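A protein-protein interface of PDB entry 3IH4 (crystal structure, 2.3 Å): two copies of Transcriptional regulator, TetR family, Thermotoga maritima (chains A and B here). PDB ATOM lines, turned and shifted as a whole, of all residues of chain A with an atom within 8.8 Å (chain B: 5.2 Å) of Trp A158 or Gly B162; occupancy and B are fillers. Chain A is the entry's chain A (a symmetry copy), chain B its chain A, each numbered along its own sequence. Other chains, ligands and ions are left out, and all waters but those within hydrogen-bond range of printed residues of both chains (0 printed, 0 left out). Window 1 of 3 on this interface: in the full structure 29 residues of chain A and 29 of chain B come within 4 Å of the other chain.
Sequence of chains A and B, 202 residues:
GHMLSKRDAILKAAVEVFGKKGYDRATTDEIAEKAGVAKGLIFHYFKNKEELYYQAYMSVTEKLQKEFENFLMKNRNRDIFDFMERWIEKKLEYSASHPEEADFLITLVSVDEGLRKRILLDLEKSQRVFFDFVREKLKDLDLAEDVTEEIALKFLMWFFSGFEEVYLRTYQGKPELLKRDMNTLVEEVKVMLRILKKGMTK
The side-chain carboxylate (OE2) of Glu A165 lies close to the side-chain carboxylate (OE2) of Glu B165, at 2.8 Å.
CG2 of Ile A151 touches CE of Met B192, 3.8 Å away. Lys A154 touches Met B192 (CD to CE, 3.7 Å). CD1 of Phe B159 touches CZ of Phe A155 (3.97 Å). Gly B162 touches Trp A158 (C to CZ2, 3.7 Å). CG2 of Val B166 touches NE1 of Trp A158, at 3.5 Å. CZ3 of Trp A158 touches SD of Met B192, 3.8 Å away. Trp B158 touches Phe A159 (CZ3 to CE1, 3.2 Å). CZ2 of Trp B158 touches C of Gly A162, 3.7 Å away. Phe A163 touches Trp B158 (N to CZ2, 3.2 Å). Val A166 touches Trp B158.
Of the printed residues of chain B, Trp A158 touches Phe B159 (3.2 Å), Gly B162 (3.7 Å), Phe B163 (3.2 Å), Val B166 (3.5 Å) and Met B192 (3.8 Å). Of the printed residues of chain A, Gly B162 touches Trp A158. No residue of chain A comes within 4 Å of Ser B161. Of the printed residues of chain A, Met B192 touches Ile A151 (3.8 Å), Lys A154 (3.7 Å), Phe A155 (3.5 Å) and Trp A158 (3.8 Å). Printed residues of chain B within 4 Å of Val A166: Trp B158 (3.5 Å). Of the printed residues of chain B, Phe A159 touches Trp B158 (3.2 Å). Of the printed residues of chain A, Phe B163 touches Trp A158. Of the printed residues of chain B, Glu A165 touches Glu B165 (2.8 Å). Ser A161 touches none of the printed residues of chain B. The nearest printed residue of chain A that does not touch Gly B162 is Val A166 (6.5 Å).
Of the 22 printed residues of chain A, 9 touch a printed residue of chain B. Hydrophobic or aromatic side chains of chain A that line the printed part of chain B: Ile A151, Phe A155, Trp A158, Phe A159, Phe A163 and Val A166. Along chain A the printed residues that touch a printed residue of chain B span positions 151 to 166. Of the 11 printed residues of chain B, 7 touch a printed residue of chain A. Among the printed residues, 14 pairs touch across the chains. Among the printed residues, no Asp or Glu carboxylate lies within 4 Å of a Lys or Arg side-chain nitrogen of the other chain.
Trp A158 touches Phe B159, and with the chains exchanged Phe A159 touches Trp B158. Trp A158 touches Gly B162, and with the chains exchanged Gly A162 touches Trp B158. Trp A158 touches Val B166, and with the chains exchanged Val A166 touches Trp B158. Glu B165 touches its own counterpart, Glu A165. Positions printed for both chains: 157, 158, 159, 160, 161, 162, 163, 164, 165 and 166. Of the 14 pairs that touch across the chains among the printed residues, 9 have their exchanged pair printed and touching as well.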
ATOM      1  N   MET A  84      -7.179  -8.167  16.900  1.00  0.00           N
ATOM      2  CA  MET A  84      -6.569  -8.966  15.816  1.00  0.00           C
ATOM      3  C   MET A  84      -7.497 -10.013  15.186  1.00  0.00           C
ATOM      4  O   MET A  84      -7.611 -10.081  13.973  1.00  0.00           O
ATOM      5  CB  MET A  84      -5.296  -9.643  16.310  1.00  0.00           C
ATOM      6  CG  MET A  84      -4.123  -8.673  16.473  1.00  0.00           C
ATOM      7  SD  MET A  84      -2.490  -9.561  17.216  1.00  0.00           S
ATOM      8  CE  MET A  84      -2.376 -10.974  15.871  1.00  0.00           C
ATOM      9  N   ILE A  88      -8.526 -10.062  11.357  1.00  0.00           N
ATOM     10  CA  ILE A  88      -8.296 -11.228  10.533  1.00  0.00           C
ATOM     11  C   ILE A  88      -9.582 -11.725   9.846  1.00  0.00           C
ATOM     12  O   ILE A  88      -9.605 -11.968   8.641  1.00  0.00           O
ATOM     13  CB  ILE A  88      -7.611 -12.346  11.347  1.00  0.00           C
ATOM     14  CG1 ILE A  88      -6.135 -11.974  11.591  1.00  0.00           C
ATOM     15  CG2 ILE A  88      -7.732 -13.683  10.634  1.00  0.00           C
ATOM     16  CD1 ILE A  88      -5.377 -12.981  12.430  1.00  0.00           C
ATOM     17  N   PHE A 130      -0.235  -0.035  12.129  1.00  0.00           N
ATOM     18  CA  PHE A 130      -0.688  -1.215  12.863  1.00  0.00           C
ATOM     19  C   PHE A 130       0.374  -1.719  13.851  1.00  0.00           C
ATOM     20  O   PHE A 130       0.065  -2.063  15.008  1.00  0.00           O
ATOM     21  CB  PHE A 130      -1.068  -2.327  11.899  1.00  0.00           C
ATOM     22  CG  PHE A 130      -1.565  -3.576  12.573  1.00  0.00           C
ATOM     23  CD1 PHE A 130      -2.611  -3.525  13.496  1.00  0.00           C
ATOM     24  CD2 PHE A 130      -1.002  -4.796  12.297  1.00  0.00           C
ATOM     25  CE1 PHE A 130      -3.080  -4.654  14.121  1.00  0.00           C
ATOM     26  CE2 PHE A 130      -1.486  -5.945  12.929  1.00  0.00           C
ATOM     27  CZ  PHE A 130      -2.528  -5.854  13.844  1.00  0.00           C
ATOM     28  N   PHE A 131       1.619  -1.770  13.384  1.00  0.00           N
ATOM     29  CA  PHE A 131       2.761  -2.134  14.228  1.00  0.00           C
ATOM     30  C   PHE A 131       2.847  -1.298  15.483  1.00  0.00           C
ATOM     31  O   PHE A 131       3.040  -1.836  16.574  1.00  0.00           O
ATOM     32  CB  PHE A 131       4.060  -1.969  13.455  1.00  0.00           C
ATOM     33  CG  PHE A 131       5.288  -2.339  14.233  1.00  0.00           C
ATOM     34  CD1 PHE A 131       5.714  -3.655  14.293  1.00  0.00           C
ATOM     35  CD2 PHE A 131       6.034  -1.366  14.894  1.00  0.00           C
ATOM     36  CE1 PHE A 131       6.842  -3.992  14.984  1.00  0.00           C
ATOM     37  CE2 PHE A 131       7.169  -1.706  15.581  1.00  0.00           C
ATOM     38  CZ  PHE A 131       7.568  -3.025  15.627  1.00  0.00           C
ATOM     39  N   VAL A 134      -0.164  -2.076  18.126  1.00  0.00           N
ATOM     40  CA  VAL A 134       0.080  -3.316  18.876  1.00  0.00           C
ATOM     41  C   VAL A 134       1.134  -3.083  19.986  1.00  0.00           C
ATOM     42  O   VAL A 134       0.958  -3.478  21.143  1.00  0.00           O
ATOM     43  CB  VAL A 134       0.510  -4.496  17.903  1.00  0.00           C
ATOM     44  CG1 VAL A 134       0.681  -5.800  18.631  1.00  0.00           C
ATOM     45  CG2 VAL A 134      -0.500  -4.691  16.803  1.00  0.00           C
ATOM     46  N   ILE A 151       9.529  -9.838  22.424  1.00  0.00           N
ATOM     47  CA  ILE A 151       9.237 -11.166  21.879  1.00  0.00           C
ATOM     48  C   ILE A 151       7.729 -11.273  21.576  1.00  0.00           C
ATOM     49  O   ILE A 151       7.356 -11.811  20.552  1.00  0.00           O
ATOM     50  CB  ILE A 151       9.762 -12.317  22.765  1.00  0.00           C
ATOM     51  CG1 ILE A 151      11.279 -12.302  22.779  1.00  0.00           C
ATOM     52  CG2 ILE A 151       9.320 -13.715  22.225  1.00  0.00           C
ATOM     53  N   ALA A 152       6.911 -10.690  22.449  1.00  0.00           N
ATOM     54  CA  ALA A 152       5.481 -10.610  22.270  1.00  0.00           C
ATOM     55  C   ALA A 152       5.124  -9.924  20.987  1.00  0.00           C
ATOM     56  O   ALA A 152       4.341 -10.449  20.217  1.00  0.00           O
ATOM     57  CB  ALA A 152       4.843  -9.878  23.412  1.00  0.00           C
ATOM     58  N   LEU A 153       5.692  -8.745  20.752  1.00  0.00           N
ATOM     59  CA  LEU A 153       5.369  -7.970  19.560  1.00  0.00           C
ATOM     60  C   LEU A 153       5.763  -8.785  18.330  1.00  0.00           C
ATOM     61  O   LEU A 153       4.972  -8.973  17.421  1.00  0.00           O
ATOM     62  CB  LEU A 153       6.081  -6.605  19.601  1.00  0.00           C
ATOM     63  CG  LEU A 153       5.868  -5.631  18.431  1.00  0.00           C
ATOM     64  CD1 LEU A 153       4.460  -5.031  18.411  1.00  0.00           C
ATOM     65  CD2 LEU A 153       6.917  -4.510  18.474  1.00  0.00           C
ATOM     66  N   LYS A 154       6.987  -9.297  18.351  1.00  0.00           N
ATOM     67  CA  LYS A 154       7.518 -10.092  17.269  1.00  0.00           C
ATOM     68  C   LYS A 154       6.628 -11.300  16.970  1.00  0.00           C
ATOM     69  O   LYS A 154       6.213 -11.472  15.845  1.00  0.00           O
ATOM     70  CB  LYS A 154       8.932 -10.541  17.607  1.00  0.00           C
ATOM     71  CG  LYS A 154       9.783 -10.865  16.400  1.00  0.00           C
ATOM     72  CD  LYS A 154      11.065 -11.598  16.818  1.00  0.00           C
ATOM     73  CE  LYS A 154      12.122 -11.623  15.681  1.00  0.00           C
ATOM     74  NZ  LYS A 154      13.402 -10.922  16.047  1.00  0.00           N
ATOM     75  N   PHE A 155       6.316 -12.106  17.983  1.00  0.00           N
ATOM     76  CA  PHE A 155       5.460 -13.286  17.817  1.00  0.00           C
ATOM     77  C   PHE A 155       4.073 -12.945  17.252  1.00  0.00           C
ATOM     78  O   PHE A 155       3.562 -13.602  16.330  1.00  0.00           O
ATOM     79  CB  PHE A 155       5.301 -14.027  19.165  1.00  0.00           C
ATOM     80  CG  PHE A 155       5.055 -15.520  19.046  1.00  0.00           C
ATOM     81  CD1 PHE A 155       4.761 -16.130  17.827  1.00  0.00           C
ATOM     82  CD2 PHE A 155       5.112 -16.315  20.175  1.00  0.00           C
ATOM     83  CE1 PHE A 155       4.536 -17.520  17.744  1.00  0.00           C
ATOM     84  CE2 PHE A 155       4.900 -17.714  20.093  1.00  0.00           C
ATOM     85  CZ  PHE A 155       4.610 -18.296  18.874  1.00  0.00           C
ATOM     86  N   LEU A 156       3.472 -11.904  17.801  1.00  0.00           N
ATOM     87  CA  LEU A 156       2.146 -11.486  17.384  1.00  0.00           C
ATOM     88  C   LEU A 156       2.117 -11.001  15.940  1.00  0.00           C
ATOM     89  O   LEU A 156       1.149 -11.284  15.223  1.00  0.00           O
ATOM     90  CB  LEU A 156       1.610 -10.392  18.313  1.00  0.00           C
ATOM     91  CG  LEU A 156       1.161 -10.843  19.705  1.00  0.00           C
ATOM     92  CD1 LEU A 156       0.779  -9.623  20.569  1.00  0.00           C
ATOM     93  CD2 LEU A 156      -0.007 -11.849  19.577  1.00  0.00           C
ATOM     94  N   MET A 157       3.146 -10.230  15.547  1.00  0.00           N
ATOM     95  CA  MET A 157       3.251  -9.701  14.184  1.00  0.00           C
ATOM     96  C   MET A 157       3.512 -10.814  13.180  1.00  0.00           C
ATOM     97  O   MET A 157       2.957 -10.815  12.116  1.00  0.00           O
ATOM     98  CB  MET A 157       4.327  -8.613  14.080  1.00  0.00           C
ATOM     99  CG  MET A 157       4.036  -7.312  14.867  1.00  0.00           C
ATOM    100  SD  MET A 157       2.422  -6.397  14.230  1.00  0.00           S
ATOM    101  CE  MET A 157       1.011  -7.255  15.285  1.00  0.00           C
ATOM    102  N   TRP A 158       4.350 -11.762  13.557  1.00  0.00           N
ATOM    103  CA  TRP A 158       4.626 -12.929  12.736  1.00  0.00           C
ATOM    104  C   TRP A 158       3.386 -13.823  12.558  1.00  0.00           C
ATOM    105  O   TRP A 158       3.160 -14.334  11.482  1.00  0.00           O
ATOM    106  CB  TRP A 158       5.803 -13.681  13.345  1.00  0.00           C
ATOM    107  CG  TRP A 158       6.133 -14.954  12.695  1.00  0.00           C
ATOM    108  CD1 TRP A 158       6.030 -15.270  11.364  1.00  0.00           C
ATOM    109  CD2 TRP A 158       6.646 -16.107  13.345  1.00  0.00           C
ATOM    110  NE1 TRP A 158       6.432 -16.571  11.161  1.00  0.00           N
ATOM    111  CE2 TRP A 158       6.820 -17.102  12.364  1.00  0.00           C
ATOM    112  CE3 TRP A 158       6.972 -16.398  14.662  1.00  0.00           C
ATOM    113  CZ2 TRP A 158       7.305 -18.356  12.667  1.00  0.00           C
ATOM    114  CZ3 TRP A 158       7.449 -17.639  14.959  1.00  0.00           C
ATOM    115  CH2 TRP A 158       7.616 -18.607  13.970  1.00  0.00           C
ATOM    116  N   PHE A 159       2.590 -13.998  13.610  1.00  0.00           N
ATOM    117  CA  PHE A 159       1.301 -14.703  13.531  1.00  0.00           C
ATOM    118  C   PHE A 159       0.308 -13.991  12.598  1.00  0.00           C
ATOM    119  O   PHE A 159      -0.296 -14.608  11.717  1.00  0.00           O
ATOM    120  CB  PHE A 159       0.651 -14.838  14.919  1.00  0.00           C
ATOM    121  CG  PHE A 159      -0.696 -15.505  14.883  1.00  0.00           C
ATOM    122  CD1 PHE A 159      -0.813 -16.864  15.065  1.00  0.00           C
ATOM    123  CD2 PHE A 159      -1.839 -14.787  14.618  1.00  0.00           C
ATOM    124  CE1 PHE A 159      -2.068 -17.477  14.997  1.00  0.00           C
ATOM    125  CE2 PHE A 159      -3.063 -15.397  14.558  1.00  0.00           C
ATOM    126  CZ  PHE A 159      -3.174 -16.733  14.753  1.00  0.00           C
ATOM    127  N   PHE A 160       0.104 -12.712  12.847  1.00  0.00           N
ATOM    128  CA  PHE A 160      -0.785 -11.922  12.041  1.00  0.00           C
ATOM    129  C   PHE A 160      -0.399 -11.941  10.547  1.00  0.00           C
ATOM    130  O   PHE A 160      -1.220 -12.246   9.685  1.00  0.00           O
ATOM    131  CB  PHE A 160      -0.817 -10.489  12.564  1.00  0.00           C
ATOM    132  CG  PHE A 160      -1.499  -9.564  11.643  1.00  0.00           C
ATOM    133  CD1 PHE A 160      -2.883  -9.630  11.491  1.00  0.00           C
ATOM    134  CD2 PHE A 160      -0.775  -8.676  10.863  1.00  0.00           C
ATOM    135  CE1 PHE A 160      -3.534  -8.813  10.593  1.00  0.00           C
ATOM    136  CE2 PHE A 160      -1.428  -7.831   9.961  1.00  0.00           C
ATOM    137  CZ  PHE A 160      -2.804  -7.908   9.829  1.00  0.00           C
ATOM    138  N   SER A 161       0.854 -11.646  10.240  1.00  0.00           N
ATOM    139  CA  SER A 161       1.299 -11.537   8.855  1.00  0.00           C
ATOM    140  C   SER A 161       1.628 -12.890   8.195  1.00  0.00           C
ATOM    141  O   SER A 161       1.512 -13.020   6.986  1.00  0.00           O
ATOM    142  CB  SER A 161       2.528 -10.631   8.779  1.00  0.00           C
ATOM    143  OG  SER A 161       3.707 -11.394   8.670  1.00  0.00           O
ATOM    144  N   GLY A 162       2.072 -13.873   8.971  1.00  0.00           N
ATOM    145  CA  GLY A 162       2.268 -15.214   8.437  1.00  0.00           C
ATOM    146  C   GLY A 162       0.976 -15.971   8.120  1.00  0.00           C
ATOM    147  O   GLY A 162       0.928 -16.776   7.195  1.00  0.00           O
ATOM    148  N   PHE A 163      -0.061 -15.740   8.915  1.00  0.00           N
ATOM    149  CA  PHE A 163      -1.361 -16.349   8.696  1.00  0.00           C
ATOM    150  C   PHE A 163      -1.964 -15.904   7.369  1.00  0.00           C
ATOM    151  O   PHE A 163      -2.609 -16.683   6.682  1.00  0.00           O
ATOM    152  CB  PHE A 163      -2.313 -15.942   9.828  1.00  0.00           C
ATOM    153  CG  PHE A 163      -3.703 -16.493   9.691  1.00  0.00           C
ATOM    154  CD1 PHE A 163      -4.004 -17.776  10.143  1.00  0.00           C
ATOM    155  CD2 PHE A 163      -4.732 -15.715   9.134  1.00  0.00           C
ATOM    156  CE1 PHE A 163      -5.297 -18.279  10.016  1.00  0.00           C
ATOM    157  CE2 PHE A 163      -6.010 -16.204   9.006  1.00  0.00           C
ATOM    158  CZ  PHE A 163      -6.298 -17.490   9.444  1.00  0.00           C
ATOM    159  N   GLU A 164      -1.811 -14.616   7.075  1.00  0.00           N
ATOM    160  CA  GLU A 164      -2.185 -14.032   5.799  1.00  0.00           C
ATOM    161  C   GLU A 164      -1.391 -14.611   4.643  1.00  0.00           C
ATOM    162  O   GLU A 164      -1.968 -15.005   3.656  1.00  0.00           O
ATOM    163  CB  GLU A 164      -1.952 -12.538   5.856  1.00  0.00           C
ATOM    164  CG  GLU A 164      -2.332 -11.814   4.611  1.00  0.00           C
ATOM    165  CD  GLU A 164      -2.273 -10.293   4.786  1.00  0.00           C
ATOM    166  OE1 GLU A 164      -1.228  -9.754   5.245  1.00  0.00           O
ATOM    167  OE2 GLU A 164      -3.293  -9.652   4.450  1.00  0.00           O
ATOM    168  N   GLU A 165      -0.074 -14.672   4.768  1.00  0.00           N
ATOM    169  CA  GLU A 165       0.749 -15.290   3.735  1.00  0.00           C
ATOM    170  C   GLU A 165       0.240 -16.712   3.460  1.00  0.00           C
ATOM    171  O   GLU A 165       0.048 -17.077   2.289  1.00  0.00           O
ATOM    172  CB  GLU A 165       2.257 -15.273   4.069  1.00  0.00           C
ATOM    173  CG  GLU A 165       3.190 -15.386   2.786  1.00  0.00           C
ATOM    174  CD  GLU A 165       4.735 -15.332   3.055  1.00  0.00           C
ATOM    175  OE1 GLU A 165       5.172 -14.866   4.144  1.00  0.00           O
ATOM    176  OE2 GLU A 165       5.525 -15.745   2.149  1.00  0.00           O
ATOM    177  N   VAL A 166      -0.081 -17.466   4.515  1.00  0.00           N
ATOM    178  CA  VAL A 166      -0.504 -18.835   4.322  1.00  0.00           C
ATOM    179  C   VAL A 166      -1.841 -19.031   3.591  1.00  0.00           C
ATOM    180  O   VAL A 166      -1.942 -19.903   2.744  1.00  0.00           O
ATOM    181  CB  VAL A 166      -0.511 -19.671   5.653  1.00  0.00           C
ATOM    182  CG1 VAL A 166      -1.046 -21.086   5.383  1.00  0.00           C
ATOM    183  CG2 VAL A 166       0.882 -19.741   6.252  1.00  0.00           C
ATOM    184  N   LEU A 196      -1.900 -18.074  22.219  1.00  0.00           N
ATOM    185  CA  LEU A 196      -0.867 -17.049  22.364  1.00  0.00           C
ATOM    186  C   LEU A 196      -1.091 -16.228  23.634  1.00  0.00           C
ATOM    187  O   LEU A 196      -0.162 -16.065  24.393  1.00  0.00           O
ATOM    188  CB  LEU A 196      -0.738 -16.108  21.143  1.00  0.00           C
ATOM    189  CG  LEU A 196      -0.293 -16.734  19.822  1.00  0.00           C
ATOM    190  CD1 LEU A 196      -0.277 -15.636  18.722  1.00  0.00           C
ATOM    191  CD2 LEU A 196       1.059 -17.426  19.924  1.00  0.00           C
ATOM    192  N   MET B 157       3.149 -27.004  13.349  1.00  0.00           N
ATOM    193  CA  MET B 157       3.701 -27.178  12.002  1.00  0.00           C
ATOM    194  C   MET B 157       3.856 -25.841  11.294  1.00  0.00           C
ATOM    195  O   MET B 157       4.831 -25.614  10.631  1.00  0.00           O
ATOM    196  CB  MET B 157       2.854 -28.142  11.163  1.00  0.00           C
ATOM    197  CG  MET B 157       2.836 -29.611  11.653  1.00  0.00           C
ATOM    198  SD  MET B 157       4.614 -30.437  11.611  1.00  0.00           S
ATOM    199  CE  MET B 157       5.345 -29.947  13.362  1.00  0.00           C
ATOM    200  N   TRP B 158       2.884 -24.965  11.471  1.00  0.00           N
ATOM    201  CA  TRP B 158       2.940 -23.619  10.925  1.00  0.00           C
ATOM    202  C   TRP B 158       4.071 -22.784  11.550  1.00  0.00           C
ATOM    203  O   TRP B 158       4.727 -22.040  10.852  1.00  0.00           O
ATOM    204  CB  TRP B 158       1.572 -22.970  11.100  1.00  0.00           C
ATOM    205  CG  TRP B 158       1.496 -21.560  10.704  1.00  0.00           C
ATOM    206  CD1 TRP B 158       2.169 -20.935   9.684  1.00  0.00           C
ATOM    207  CD2 TRP B 158       0.677 -20.571  11.311  1.00  0.00           C
ATOM    208  NE1 TRP B 158       1.826 -19.602   9.646  1.00  0.00           N
ATOM    209  CE2 TRP B 158       0.906 -19.359  10.633  1.00  0.00           C
ATOM    210  CE3 TRP B 158      -0.223 -20.591  12.365  1.00  0.00           C
ATOM    211  CZ2 TRP B 158       0.264 -18.190  10.980  1.00  0.00           C
ATOM    212  CZ3 TRP B 158      -0.856 -19.435  12.708  1.00  0.00           C
ATOM    213  CH2 TRP B 158      -0.616 -18.246  12.019  1.00  0.00           C
ATOM    214  N   PHE B 159       4.295 -22.917  12.854  1.00  0.00           N
ATOM    215  CA  PHE B 159       5.437 -22.292  13.540  1.00  0.00           C
ATOM    216  C   PHE B 159       6.784 -22.813  13.014  1.00  0.00           C
ATOM    217  O   PHE B 159       7.683 -22.037  12.680  1.00  0.00           O
ATOM    218  CB  PHE B 159       5.382 -22.538  15.058  1.00  0.00           C
ATOM    219  CG  PHE B 159       6.558 -21.963  15.797  1.00  0.00           C
ATOM    220  CD1 PHE B 159       6.500 -20.699  16.337  1.00  0.00           C
ATOM    221  CD2 PHE B 159       7.737 -22.661  15.910  1.00  0.00           C
ATOM    222  CE1 PHE B 159       7.611 -20.163  16.994  1.00  0.00           C
ATOM    223  CE2 PHE B 159       8.818 -22.129  16.560  1.00  0.00           C
ATOM    224  CZ  PHE B 159       8.750 -20.889  17.103  1.00  0.00           C
ATOM    225  N   PHE B 160       6.929 -24.124  13.008  1.00  0.00           N
ATOM    226  CA  PHE B 160       8.130 -24.744  12.524  1.00  0.00           C
ATOM    227  C   PHE B 160       8.460 -24.339  11.072  1.00  0.00           C
ATOM    228  O   PHE B 160       9.561 -23.883  10.777  1.00  0.00           O
ATOM    229  CB  PHE B 160       8.008 -26.261  12.639  1.00  0.00           C
ATOM    230  CG  PHE B 160       9.086 -26.973  11.931  1.00  0.00           C
ATOM    231  CD1 PHE B 160      10.382 -26.953  12.440  1.00  0.00           C
ATOM    232  CD2 PHE B 160       8.846 -27.599  10.718  1.00  0.00           C
ATOM    233  CE1 PHE B 160      11.415 -27.564  11.764  1.00  0.00           C
ATOM    234  CE2 PHE B 160       9.884 -28.237  10.031  1.00  0.00           C
ATOM    235  CZ  PHE B 160      11.164 -28.211  10.558  1.00  0.00           C
ATOM    236  N   SER B 161       7.500 -24.476  10.172  1.00  0.00           N
ATOM    237  CA  SER B 161       7.735 -24.217   8.755  1.00  0.00           C
ATOM    238  C   SER B 161       7.660 -22.728   8.369  1.00  0.00           C
ATOM    239  O   SER B 161       8.301 -22.314   7.416  1.00  0.00           O
ATOM    240  CB  SER B 161       6.728 -25.004   7.914  1.00  0.00           C
ATOM    241  OG  SER B 161       5.682 -24.169   7.475  1.00  0.00           O
ATOM    242  N   GLY B 162       6.856 -21.939   9.075  1.00  0.00           N
ATOM    243  CA  GLY B 162       6.843 -20.499   8.855  1.00  0.00           C
ATOM    244  C   GLY B 162       8.092 -19.766   9.350  1.00  0.00           C
ATOM    245  O   GLY B 162       8.504 -18.763   8.773  1.00  0.00           O
ATOM    246  N   PHE B 163       8.670 -20.244  10.444  1.00  0.00           N
ATOM    247  CA  PHE B 163       9.891 -19.678  10.991  1.00  0.00           C
ATOM    248  C   PHE B 163      11.053 -19.821  10.016  1.00  0.00           C
ATOM    249  O   PHE B 163      11.891 -18.938   9.906  1.00  0.00           O
ATOM    250  CB  PHE B 163      10.252 -20.404  12.293  1.00  0.00           C
ATOM    251  CG  PHE B 163      11.520 -19.920  12.937  1.00  0.00           C
ATOM    252  CD1 PHE B 163      11.507 -18.805  13.774  1.00  0.00           C
ATOM    253  CD2 PHE B 163      12.733 -20.598  12.733  1.00  0.00           C
ATOM    254  CE1 PHE B 163      12.686 -18.364  14.370  1.00  0.00           C
ATOM    255  CE2 PHE B 163      13.900 -20.169  13.319  1.00  0.00           C
ATOM    256  CZ  PHE B 163      13.882 -19.047  14.138  1.00  0.00           C
ATOM    257  N   GLU B 164      11.126 -20.987   9.379  1.00  0.00           N
ATOM    258  CA  GLU B 164      12.069 -21.264   8.311  1.00  0.00           C
ATOM    259  C   GLU B 164      11.849 -20.375   7.101  1.00  0.00           C
ATOM    260  O   GLU B 164      12.785 -19.787   6.610  1.00  0.00           O
ATOM    261  CB  GLU B 164      11.924 -22.711   7.891  1.00  0.00           C
ATOM    262  CG  GLU B 164      12.867 -23.130   6.817  1.00  0.00           C
ATOM    263  CD  GLU B 164      12.825 -24.642   6.570  1.00  0.00           C
ATOM    264  OE1 GLU B 164      11.719 -25.214   6.361  1.00  0.00           O
ATOM    265  OE2 GLU B 164      13.923 -25.241   6.586  1.00  0.00           O
ATOM    266  N   GLU B 165      10.616 -20.269   6.629  1.00  0.00           N
ATOM    267  CA  GLU B 165      10.313 -19.370   5.522  1.00  0.00           C
ATOM    268  C   GLU B 165      10.806 -17.957   5.861  1.00  0.00           C
ATOM    269  O   GLU B 165      11.483 -17.329   5.032  1.00  0.00           O
ATOM    270  CB  GLU B 165       8.820 -19.379   5.124  1.00  0.00           C
ATOM    271  CG  GLU B 165       8.561 -18.901   3.629  1.00  0.00           C
ATOM    272  CD  GLU B 165       7.068 -18.928   3.150  1.00  0.00           C
ATOM    273  OE1 GLU B 165       6.214 -19.618   3.774  1.00  0.00           O
ATOM    274  OE2 GLU B 165       6.748 -18.260   2.116  1.00  0.00           O
ATOM    275  N   VAL B 166      10.571 -17.502   7.096  1.00  0.00           N
ATOM    276  CA  VAL B 166      10.954 -16.155   7.455  1.00  0.00           C
ATOM    277  C   VAL B 166      12.463 -15.867   7.478  1.00  0.00           C
ATOM    278  O   VAL B 166      12.883 -14.822   7.008  1.00  0.00           O
ATOM    279  CB  VAL B 166      10.311 -15.671   8.804  1.00  0.00           C
ATOM    280  CG1 VAL B 166      10.825 -14.266   9.158  1.00  0.00           C
ATOM    281  CG2 VAL B 166       8.796 -15.666   8.707  1.00  0.00           C
ATOM    282  N   MET B 192       9.474 -18.469  22.451  1.00  0.00           N
ATOM    283  CA  MET B 192       8.273 -18.713  21.629  1.00  0.00           C
ATOM    284  C   MET B 192       7.736 -20.124  21.680  1.00  0.00           C
ATOM    285  O   MET B 192       6.532 -20.298  21.774  1.00  0.00           O
ATOM    286  CB  MET B 192       8.497 -18.322  20.180  1.00  0.00           C
ATOM    287  CG  MET B 192       8.698 -16.845  20.042  1.00  0.00           C
ATOM    288  SD  MET B 192       8.971 -16.261  18.182  1.00  0.00           S
ATOM    289  CE  MET B 192       9.991 -14.634  18.609  1.00  0.00           C
